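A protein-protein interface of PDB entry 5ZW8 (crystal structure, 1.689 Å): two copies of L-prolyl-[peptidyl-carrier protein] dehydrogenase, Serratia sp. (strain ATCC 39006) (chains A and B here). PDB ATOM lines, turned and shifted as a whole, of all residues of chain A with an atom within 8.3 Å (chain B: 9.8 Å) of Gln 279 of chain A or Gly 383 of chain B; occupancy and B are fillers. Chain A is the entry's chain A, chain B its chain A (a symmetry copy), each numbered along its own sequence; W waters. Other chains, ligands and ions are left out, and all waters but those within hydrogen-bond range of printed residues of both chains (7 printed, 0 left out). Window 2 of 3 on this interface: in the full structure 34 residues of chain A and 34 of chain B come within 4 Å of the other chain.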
ATOM      1  N   ALA A 267     -27.395  11.482 -14.072  1.00  0.00           N
ATOM      2  CA  ALA A 267     -26.682  12.508 -13.359  1.00  0.00           C
ATOM      3  C   ALA A 267     -27.222  12.649 -11.949  1.00  0.00           C
ATOM      4  O   ALA A 267     -26.486  13.101 -11.079  1.00  0.00           O
ATOM      5  CB  ALA A 267     -26.750  13.870 -14.102  1.00  0.00           C
ATOM      6  N   LYS A 268     -28.452  12.201 -11.717  1.00  0.00           N
ATOM      7  CA  LYS A 268     -28.995  12.229 -10.347  1.00  0.00           C
ATOM      8  C   LYS A 268     -28.575  11.011  -9.538  1.00  0.00           C
ATOM      9  O   LYS A 268     -28.518  11.100  -8.298  1.00  0.00           O
ATOM     10  CB  LYS A 268     -30.527  12.283 -10.366  1.00  0.00           C
ATOM     11  CG  LYS A 268     -31.058  13.569 -10.964  1.00  0.00           C
ATOM     12  CD  LYS A 268     -32.579  13.429 -11.195  1.00  0.00           C
ATOM     13  CE  LYS A 268     -33.122  14.619 -11.923  1.00  0.00           C
ATOM     14  NZ  LYS A 268     -34.545  14.435 -12.385  1.00  0.00           N
ATOM     15  N   ARG A 270     -25.797   8.699 -10.270  1.00  0.00           N
ATOM     16  CA  ARG A 270     -24.376   8.388 -10.166  1.00  0.00           C
ATOM     17  C   ARG A 270     -23.695   9.341  -9.176  1.00  0.00           C
ATOM     18  O   ARG A 270     -23.710  10.568  -9.350  1.00  0.00           O
ATOM     19  CB  ARG A 270     -23.744   8.455 -11.560  1.00  0.00           C
ATOM     20  CG  ARG A 270     -22.253   8.548 -11.568  1.00  0.00           C
ATOM     21  CD  ARG A 270     -21.661   7.282 -11.029  1.00  0.00           C
ATOM     22  NE  ARG A 270     -20.172   7.211 -11.264  1.00  0.00           N
ATOM     23  CZ  ARG A 270     -19.459   6.139 -10.918  1.00  0.00           C
ATOM     24  NH1 ARG A 270     -20.039   5.131 -10.287  1.00  0.00           N
ATOM     25  NH2 ARG A 270     -18.207   6.048 -11.215  1.00  0.00           N
ATOM     26  N   GLN A 271     -23.085   8.787  -8.113  1.00  0.00           N
ATOM     27  CA  GLN A 271     -22.380   9.586  -7.117  1.00  0.00           C
ATOM     28  C   GLN A 271     -20.879   9.440  -7.278  1.00  0.00           C
ATOM     29  O   GLN A 271     -20.399   8.330  -7.455  1.00  0.00           O
ATOM     30  CB  GLN A 271     -22.745   9.148  -5.690  1.00  0.00           C
ATOM     31  CG  GLN A 271     -24.172   8.818  -5.552  1.00  0.00           C
ATOM     32  CD  GLN A 271     -24.896   9.971  -4.983  1.00  0.00           C
ATOM     33  OE1 GLN A 271     -25.910  10.421  -5.526  1.00  0.00           O
ATOM     34  NE2 GLN A 271     -24.391  10.476  -3.872  1.00  0.00           N
ATOM     35  N   GLN A 272     -20.155  10.553  -7.147  1.00  0.00           N
ATOM     36  CA  GLN A 272     -18.714  10.577  -6.913  1.00  0.00           C
ATOM     37  C   GLN A 272     -18.421  11.699  -5.928  1.00  0.00           C
ATOM     38  O   GLN A 272     -19.123  12.727  -5.919  1.00  0.00           O
ATOM     39  CB  GLN A 272     -17.892  10.848  -8.216  1.00  0.00           C
ATOM     40  CG  GLN A 272     -17.958   9.701  -9.213  1.00  0.00           C
ATOM     41  CD  GLN A 272     -17.109   8.490  -8.684  1.00  0.00           C
ATOM     42  OE1 GLN A 272     -15.905   8.467  -8.873  1.00  0.00           O
ATOM     43  NE2 GLN A 272     -17.754   7.532  -8.037  1.00  0.00           N
ATOM     44  N   GLY A 274     -19.048  11.819  -2.940  1.00  0.00           N
ATOM     45  CA  GLY A 274     -20.107  11.883  -1.959  1.00  0.00           C
ATOM     46  C   GLY A 274     -21.333  12.644  -2.394  1.00  0.00           C
ATOM     47  O   GLY A 274     -22.191  12.949  -1.568  1.00  0.00           O
ATOM     48  N   LYS A 275     -21.489  12.923  -3.688  1.00  0.00           N
ATOM     49  CA  LYS A 275     -22.688  13.626  -4.144  1.00  0.00           C
ATOM     50  C   LYS A 275     -22.995  13.196  -5.566  1.00  0.00           C
ATOM     51  O   LYS A 275     -22.161  12.570  -6.233  1.00  0.00           O
ATOM     52  CB  LYS A 275     -22.511  15.132  -4.100  1.00  0.00           C
ATOM     53  CG  LYS A 275     -21.488  15.619  -5.098  1.00  0.00           C
ATOM     54  CD  LYS A 275     -21.100  17.062  -4.732  1.00  0.00           C
ATOM     55  CE  LYS A 275     -20.097  16.972  -3.630  1.00  0.00           C
ATOM     56  NZ  LYS A 275     -19.991  18.220  -2.844  1.00  0.00           N
ATOM     57  N   ALA A 276     -24.241  13.447  -5.987  1.00  0.00           N
ATOM     58  CA  ALA A 276     -24.626  13.177  -7.383  1.00  0.00           C
ATOM     59  C   ALA A 276     -23.734  13.986  -8.353  1.00  0.00           C
ATOM     60  O   ALA A 276     -23.388  15.124  -8.085  1.00  0.00           O
ATOM     61  CB  ALA A 276     -26.097  13.528  -7.595  1.00  0.00           C
ATOM     62  N   ILE A 277     -23.317  13.372  -9.478  1.00  0.00           N
ATOM     63  CA  ILE A 277     -22.392  14.101 -10.363  1.00  0.00           C
ATOM     64  C   ILE A 277     -23.080  15.313 -10.968  1.00  0.00           C
ATOM     65  O   ILE A 277     -22.387  16.257 -11.351  1.00  0.00           O
ATOM     66  CB  ILE A 277     -21.847  13.220 -11.515  1.00  0.00           C
ATOM     67  CG1 ILE A 277     -23.023  12.609 -12.296  1.00  0.00           C
ATOM     68  CG2 ILE A 277     -20.751  12.161 -10.924  1.00  0.00           C
ATOM     69  CD1 ILE A 277     -22.520  11.854 -13.622  1.00  0.00           C
ATOM     70  N   GLY A 278     -24.422  15.318 -11.011  1.00  0.00           N
ATOM     71  CA  GLY A 278     -25.129  16.515 -11.512  1.00  0.00           C
ATOM     72  C   GLY A 278     -24.932  17.749 -10.641  1.00  0.00           C
ATOM     73  O   GLY A 278     -25.235  18.866 -11.091  1.00  0.00           O
ATOM     74  N   GLN A 279     -24.430  17.574  -9.418  1.00  0.00           N
ATOM     75  CA  GLN A 279     -24.187  18.709  -8.510  1.00  0.00           C
ATOM     76  C   GLN A 279     -22.944  19.490  -8.882  1.00  0.00           C
ATOM     77  O   GLN A 279     -22.752  20.606  -8.392  1.00  0.00           O
ATOM     78  CB  GLN A 279     -24.005  18.236  -7.053  1.00  0.00           C
ATOM     79  CG  GLN A 279     -25.254  17.443  -6.566  1.00  0.00           C
ATOM     80  CD  GLN A 279     -26.152  18.255  -5.683  1.00  0.00           C
ATOM     81  OE1 GLN A 279     -26.130  19.489  -5.715  1.00  0.00           O
ATOM     82  NE2 GLN A 279     -26.901  17.571  -4.831  1.00  0.00           N
ATOM     83  N   PHE A 280     -22.044  18.929  -9.709  1.00  0.00           N
ATOM     84  CA  PHE A 280     -20.881  19.690 -10.190  1.00  0.00           C
ATOM     85  C   PHE A 280     -21.303  20.541 -11.390  1.00  0.00           C
ATOM     86  O   PHE A 280     -21.921  20.027 -12.337  1.00  0.00           O
ATOM     87  CB  PHE A 280     -19.781  18.723 -10.634  1.00  0.00           C
ATOM     88  CG  PHE A 280     -19.266  17.912  -9.494  1.00  0.00           C
ATOM     89  CD1 PHE A 280     -18.524  18.546  -8.516  1.00  0.00           C
ATOM     90  CD2 PHE A 280     -19.495  16.531  -9.433  1.00  0.00           C
ATOM     91  CE1 PHE A 280     -18.004  17.808  -7.380  1.00  0.00           C
ATOM     92  CE2 PHE A 280     -18.990  15.803  -8.280  1.00  0.00           C
ATOM     93  CZ  PHE A 280     -18.281  16.446  -7.289  1.00  0.00           C
ATOM     94  N   GLN A 281     -20.961  21.825 -11.366  1.00  0.00           N
ATOM     95  CA  GLN A 281     -21.438  22.695 -12.458  1.00  0.00           C
ATOM     96  C   GLN A 281     -20.869  22.270 -13.821  1.00  0.00           C
ATOM     97  O   GLN A 281     -21.531  22.500 -14.847  1.00  0.00           O
ATOM     98  CB  GLN A 281     -21.159  24.177 -12.147  1.00  0.00           C
ATOM     99  CG  GLN A 281     -22.093  24.615 -11.009  1.00  0.00           C
ATOM    100  CD  GLN A 281     -21.737  25.971 -10.471  1.00  0.00           C
ATOM    101  OE1 GLN A 281     -20.760  26.597 -10.909  1.00  0.00           O
ATOM    102  NE2 GLN A 281     -22.462  26.401  -9.427  1.00  0.00           N
ATOM    103  N   SER A 282     -19.660  21.693 -13.889  1.00  0.00           N
ATOM    104  CA  SER A 282     -19.189  21.214 -15.207  1.00  0.00           C
ATOM    105  C   SER A 282     -20.187  20.220 -15.794  1.00  0.00           C
ATOM    106  O   SER A 282     -20.360  20.164 -17.021  1.00  0.00           O
ATOM    107  CB  SER A 282     -17.806  20.552 -15.097  1.00  0.00           C
ATOM    108  OG  SER A 282     -16.804  21.562 -14.941  1.00  0.00           O
ATOM    109  N   VAL A 283     -20.799  19.395 -14.941  1.00  0.00           N
ATOM    110  CA  VAL A 283     -21.746  18.372 -15.423  1.00  0.00           C
ATOM    111  C   VAL A 283     -23.112  18.993 -15.713  1.00  0.00           C
ATOM    112  O   VAL A 283     -23.700  18.784 -16.798  1.00  0.00           O
ATOM    113  CB  VAL A 283     -21.870  17.227 -14.403  1.00  0.00           C
ATOM    114  CG1 VAL A 283     -23.036  16.244 -14.790  1.00  0.00           C
ATOM    115  CG2 VAL A 283     -20.432  16.466 -14.284  1.00  0.00           C
ATOM    116  N   SER A 284     -23.635  19.747 -14.740  1.00  0.00           N
ATOM    117  CA  SER A 284     -24.984  20.284 -14.920  1.00  0.00           C
ATOM    118  C   SER A 284     -25.005  21.296 -16.054  1.00  0.00           C
ATOM    119  O   SER A 284     -26.021  21.380 -16.759  1.00  0.00           O
ATOM    120  CB  SER A 284     -25.525  20.913 -13.613  1.00  0.00           C
ATOM    121  OG  SER A 284     -24.674  21.993 -13.168  1.00  0.00           O
ATOM    122  N   ASN A 285     -23.940  22.068 -16.262  1.00  0.00           N
ATOM    123  CA  ASN A 285     -23.982  23.054 -17.359  1.00  0.00           C
ATOM    124  C   ASN A 285     -24.192  22.376 -18.724  1.00  0.00           C
ATOM    125  O   ASN A 285     -24.944  22.894 -19.564  1.00  0.00           O
ATOM    126  CB  ASN A 285     -22.696  23.900 -17.416  1.00  0.00           C
ATOM    127  CG  ASN A 285     -22.601  24.935 -16.299  1.00  0.00           C
ATOM    128  OD1 ASN A 285     -21.508  25.492 -16.008  1.00  0.00           O
ATOM    129  ND2 ASN A 285     -23.684  25.161 -15.667  1.00  0.00           N
ATOM    130  N   ILE A 287     -25.764  19.461 -19.191  1.00  0.00           N
ATOM    131  CA  ILE A 287     -27.148  18.965 -19.277  1.00  0.00           C
ATOM    132  C   ILE A 287     -28.111  20.137 -19.563  1.00  0.00           C
ATOM    133  O   ILE A 287     -29.103  20.002 -20.302  1.00  0.00           O
ATOM    134  CB  ILE A 287     -27.499  18.207 -17.991  1.00  0.00           C
ATOM    135  CG1 ILE A 287     -26.550  16.994 -17.887  1.00  0.00           C
ATOM    136  CG2 ILE A 287     -28.970  17.786 -18.001  1.00  0.00           C
ATOM    137  CD1 ILE A 287     -26.681  16.250 -16.546  1.00  0.00           C
ATOM    138  N   LYS B 372     -28.487  29.258 -14.518  1.00  0.00           N
ATOM    139  CA  LYS B 372     -28.210  27.816 -14.646  1.00  0.00           C
ATOM    140  C   LYS B 372     -28.460  27.085 -13.338  1.00  0.00           C
ATOM    141  O   LYS B 372     -28.971  25.952 -13.362  1.00  0.00           O
ATOM    142  CB  LYS B 372     -26.771  27.573 -15.137  1.00  0.00           C
ATOM    143  CG  LYS B 372     -26.640  27.968 -16.611  1.00  0.00           C
ATOM    144  CD  LYS B 372     -25.124  27.870 -17.043  1.00  0.00           C
ATOM    145  CE  LYS B 372     -24.816  28.553 -18.375  1.00  0.00           C
ATOM    146  NZ  LYS B 372     -23.405  28.154 -18.848  1.00  0.00           N
ATOM    147  N   GLU B 373     -28.097  27.690 -12.196  1.00  0.00           N
ATOM    148  CA  GLU B 373     -28.401  27.062 -10.899  1.00  0.00           C
ATOM    149  C   GLU B 373     -29.907  26.904 -10.704  1.00  0.00           C
ATOM    150  O   GLU B 373     -30.380  25.902 -10.163  1.00  0.00           O
ATOM    151  CB  GLU B 373     -27.784  27.878  -9.762  1.00  0.00           C
ATOM    152  CG  GLU B 373     -26.188  27.839  -9.807  1.00  0.00           C
ATOM    153  CD  GLU B 373     -25.634  26.353  -9.895  1.00  0.00           C
ATOM    154  OE1 GLU B 373     -25.789  25.673  -8.893  1.00  0.00           O
ATOM    155  OE2 GLU B 373     -25.256  25.955 -11.017  1.00  0.00           O
ATOM    156  N   ALA B 376     -30.964  24.072 -13.022  1.00  0.00           N
ATOM    157  CA  ALA B 376     -30.483  22.808 -12.448  1.00  0.00           C
ATOM    158  C   ALA B 376     -31.392  22.376 -11.303  1.00  0.00           C
ATOM    159  O   ALA B 376     -31.762  21.190 -11.199  1.00  0.00           O
ATOM    160  CB  ALA B 376     -29.034  22.987 -11.958  1.00  0.00           C
ATOM    161  N   ARG B 377     -31.811  23.335 -10.469  1.00  0.00           N
ATOM    162  CA  ARG B 377     -32.699  22.975  -9.357  1.00  0.00           C
ATOM    163  C   ARG B 377     -34.049  22.484  -9.888  1.00  0.00           C
ATOM    164  O   ARG B 377     -34.564  21.447  -9.425  1.00  0.00           O
ATOM    165  CB  ARG B 377     -32.861  24.173  -8.415  1.00  0.00           C
ATOM    166  CG  ARG B 377     -33.864  23.918  -7.271  1.00  0.00           C
ATOM    167  CD  ARG B 377     -33.717  25.030  -6.199  1.00  0.00           C
ATOM    168  NE  ARG B 377     -32.333  25.081  -5.667  1.00  0.00           N
ATOM    169  CZ  ARG B 377     -31.797  24.260  -4.733  1.00  0.00           C
ATOM    170  NH1 ARG B 377     -32.504  23.265  -4.153  1.00  0.00           N
ATOM    171  NH2 ARG B 377     -30.515  24.424  -4.378  1.00  0.00           N
ATOM    172  N   LYS B 378     -34.605  23.160 -10.908  1.00  0.00           N
ATOM    173  CA  LYS B 378     -35.878  22.699 -11.465  1.00  0.00           C
ATOM    174  C   LYS B 378     -35.734  21.322 -12.104  1.00  0.00           C
ATOM    175  O   LYS B 378     -36.687  20.536 -12.100  1.00  0.00           O
ATOM    176  CB  LYS B 378     -36.426  23.696 -12.486  1.00  0.00           C
ATOM    177  CG  LYS B 378     -36.788  25.044 -11.871  1.00  0.00           C
ATOM    178  CD  LYS B 378     -37.934  24.912 -10.844  1.00  0.00           C
ATOM    179  CE  LYS B 378     -38.726  26.250 -10.677  1.00  0.00           C
ATOM    180  NZ  LYS B 378     -38.066  27.311  -9.841  1.00  0.00           N
ATOM    181  N   LEU B 379     -34.548  20.997 -12.651  1.00  0.00           N
ATOM    182  CA  LEU B 379     -34.333  19.720 -13.307  1.00  0.00           C
ATOM    183  C   LEU B 379     -34.045  18.602 -12.311  1.00  0.00           C
ATOM    184  O   LEU B 379     -33.888  17.446 -12.732  1.00  0.00           O
ATOM    185  CB  LEU B 379     -33.168  19.852 -14.294  1.00  0.00           C
ATOM    186  CG  LEU B 379     -33.459  20.621 -15.602  1.00  0.00           C
ATOM    187  CD1 LEU B 379     -32.133  20.736 -16.358  1.00  0.00           C
ATOM    188  CD2 LEU B 379     -34.529  20.018 -16.481  1.00  0.00           C
ATOM    189  N   GLY B 380     -33.955  18.914 -11.026  1.00  0.00           N
ATOM    190  CA  GLY B 380     -33.702  17.918 -10.011  1.00  0.00           C
ATOM    191  C   GLY B 380     -32.254  17.603  -9.776  1.00  0.00           C
ATOM    192  O   GLY B 380     -31.958  16.563  -9.185  1.00  0.00           O
ATOM    193  N   LEU B 381     -31.326  18.468 -10.223  1.00  0.00           N
ATOM    194  CA  LEU B 381     -29.891  18.279 -10.106  1.00  0.00           C
ATOM    195  C   LEU B 381     -29.343  18.934  -8.854  1.00  0.00           C
ATOM    196  O   LEU B 381     -28.117  18.930  -8.649  1.00  0.00           O
ATOM    197  CB  LEU B 381     -29.172  18.846 -11.374  1.00  0.00           C
ATOM    198  CG  LEU B 381     -29.639  18.210 -12.681  1.00  0.00           C
ATOM    199  CD1 LEU B 381     -28.893  18.858 -13.847  1.00  0.00           C
ATOM    200  CD2 LEU B 381     -29.332  16.704 -12.619  1.00  0.00           C
ATOM    201  N   ARG B 382     -30.204  19.505  -8.004  1.00  0.00           N
ATOM    202  CA  ARG B 382     -29.677  20.131  -6.790  1.00  0.00           C
ATOM    203  C   ARG B 382     -30.261  19.465  -5.528  1.00  0.00           C
ATOM    204  O   ARG B 382     -30.655  20.141  -4.572  1.00  0.00           O
ATOM    205  CB  ARG B 382     -29.916  21.641  -6.777  1.00  0.00           C
ATOM    206  CG  ARG B 382     -29.169  22.413  -7.919  1.00  0.00           C
ATOM    207  CD  ARG B 382     -27.660  22.393  -7.625  1.00  0.00           C
ATOM    208  NE  ARG B 382     -26.877  23.030  -8.658  1.00  0.00           N
ATOM    209  CZ  ARG B 382     -26.286  22.350  -9.646  1.00  0.00           C
ATOM    210  NH1 ARG B 382     -25.513  22.985 -10.534  1.00  0.00           N
ATOM    211  NH2 ARG B 382     -26.496  21.057  -9.787  1.00  0.00           N
ATOM    212  N   GLY B 383     -30.245  18.140  -5.505  1.00  0.00           N
ATOM    213  CA  GLY B 383     -30.576  17.401  -4.292  1.00  0.00           C
ATOM    214  C   GLY B 383     -32.060  17.175  -4.282  1.00  0.00           C
ATOM    215  O   GLY B 383     -32.683  17.117  -5.348  1.00  0.00           O
HETATM  216  O   HOH W   1     -24.921  25.849 -19.822  1.00  0.00           O
HETATM  217  O   HOH W   2     -25.269  24.367 -13.697  1.00  0.00           O
HETATM  218  O   HOH W   3     -27.486  16.213  -9.260  1.00  0.00           O
HETATM  219  O   HOH W   4     -24.064  24.721  -6.965  1.00  0.00           O
HETATM  220  O   HOH W   5     -22.032  28.832 -16.693  1.00  0.00           O
HETATM  221  O   HOH W   6     -24.614  21.615  -6.568  1.00  0.00           O
HETATM  222  O   HOH W   7     -36.207  15.899 -14.389  1.00  0.00           O
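The backbone carbonyl oxygen (O) of Leu 379 of chain B sits close to the side-chain amino group (NZ) of Lys 268 of chain A (3.1 Å).
The backbone carbonyl oxygen of Gly 278 of chain A sits at hydrogen-bond distance from the guanidinium group of Arg 382 of chain B, 2.8 Å away.
The side-chain amide nitrogen (NE2) of Gln 279 of chain A lies close to the backbone NH (N) of Gly 383 of chain B (3.5 Å).
NE2 of Gln 281 of chain A lies close to OE2 of Glu 373 of chain B (3.2 Å).
The guanidinium group (NH1) of Arg 382 of chain B lies within hydrogen-bond range of the side-chain hydroxyl (OG) of Ser 284 of chain A.
The backbone NH of Gly 278 of chain A is in hydrogen-bond range of the backbone carbonyl oxygen of Ala 267 of chain A (3.0 Å).
The backbone carbonyl oxygen (O) of Phe 280 of chain A lies within hydrogen-bond range of the side-chain hydroxyl (OG) of Ser 284 of chain A (3.5 Å).
The side-chain amide oxygen of Asn 285 of chain A sits close to the backbone carbonyl oxygen of Gln 281 of chain A (3.2 Å).
The guanidinium group (NE) of Arg 382 of chain B lies within salt-bridge range of the side-chain carboxylate (OE1) of Glu 373 of chain B (2.9 Å).
The backbone NH (N) of Leu 381 of chain B sits at hydrogen-bond distance from the backbone carbonyl oxygen (O) of Ala 376 of chain B, 2.9 Å away.
Gly 380 of chain B touches Lys 268 of chain A.
Lys 268 of chain A touches Leu 381 of chain B (CG to CD2, 3.9 Å).
Gly 278 of chain A touches Leu 381 of chain B (O to O, 3.8 Å).
OE1 of Gln 279 of chain A touches O of Leu 381 of chain B, 3.6 Å away.
NH2 of Arg 382 of chain B touches CA of Gln 279 of chain A (3.5 Å).
CG of Gln 281 of chain A touches NH1 of Arg 382 of chain B, 3.8 Å away.
Leu 381 of chain B touches Ser 284 of chain A (CD1 to CB, 3.95 Å).
Lys 372 of chain B touches Asn 285 of chain A.
Of the printed residues of chain B, Gln 279 of chain A touches Leu 381 (3.6 Å), Arg 382 (3.5 Å) and Gly 383 (3.5 Å).
Gly 383 of chain B touches just one residue of chain A: Gln 279 (3.5 Å).
No residue of chain B comes within 4 Å of Ala 276 of chain A.
Gly 278 of chain A touches just these residues of chain B: Leu 381 (3.8 Å) and Arg 382 (2.8 Å).
Of the printed residues of chain A, Leu 379 of chain B touches Lys 268 (3.0 Å).
Of the printed residues of chain B, Asn 285 of chain A touches Lys 372.
Of the printed residues of chain B, Ser 284 of chain A touches Leu 381 (3.95 Å) and Arg 382 (2.9 Å).
Printed residues of chain A within 4 Å of Glu 373 of chain B: Gln 281.
Printed residues of chain A within 4 Å of Gly 380 of chain B: Lys 268 (3.6 Å).
Gln 271 of chain A touches none of the printed residues of chain B.
The nearest residue of chain B that does not touch Gln 279 of chain A is Glu 373 of chain B (5.9 Å).
The nearest residue of chain A that does not touch Gly 383 of chain B is Ala 276 of chain A (6.5 Å).
The nearest printed residue of chain A that does not touch Gly 380 of chain B is Ala 267 of chain A (6.7 Å).
Among the printed residues, no Asp or Glu carboxylate lies within 4 Å of a Lys or Arg side-chain nitrogen of the other chain.
No position is printed for both chains.
Water W2 lies within hydrogen-bond range of the side-chain hydroxyl of Ser 284 of chain A, the side-chain amide nitrogen of Asn 285 of chain A, the side-chain carboxylate of Glu 373 of chain B and the guanidinium group of Arg 382 of chain B.
Water W6 lies within hydrogen-bond range of the side-chain amide oxygen of Gln 279 of chain A (2.7 Å) and the guanidinium group of Arg 382 of chain B (3.4 Å).
Water W4 lies within hydrogen-bond range of the side-chain carboxylate of Glu 373 of chain B and the side-chain amide nitrogen of Gln 281 of chain A.
Water W3 bridges O of Leu 381 of chain B (2.9 Å) and N of Gln 279 of chain A (3.3 Å).
Water W1 bridges NZ of Lys 372 of chain B (2.9 Å) and O of Asn 285 of chain A (3.0 Å).
Water W7 lies within hydrogen-bond range of NZ of Lys 268 of chain A (3.0 Å) and O of Leu 379 of chain B (3.2 Å).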
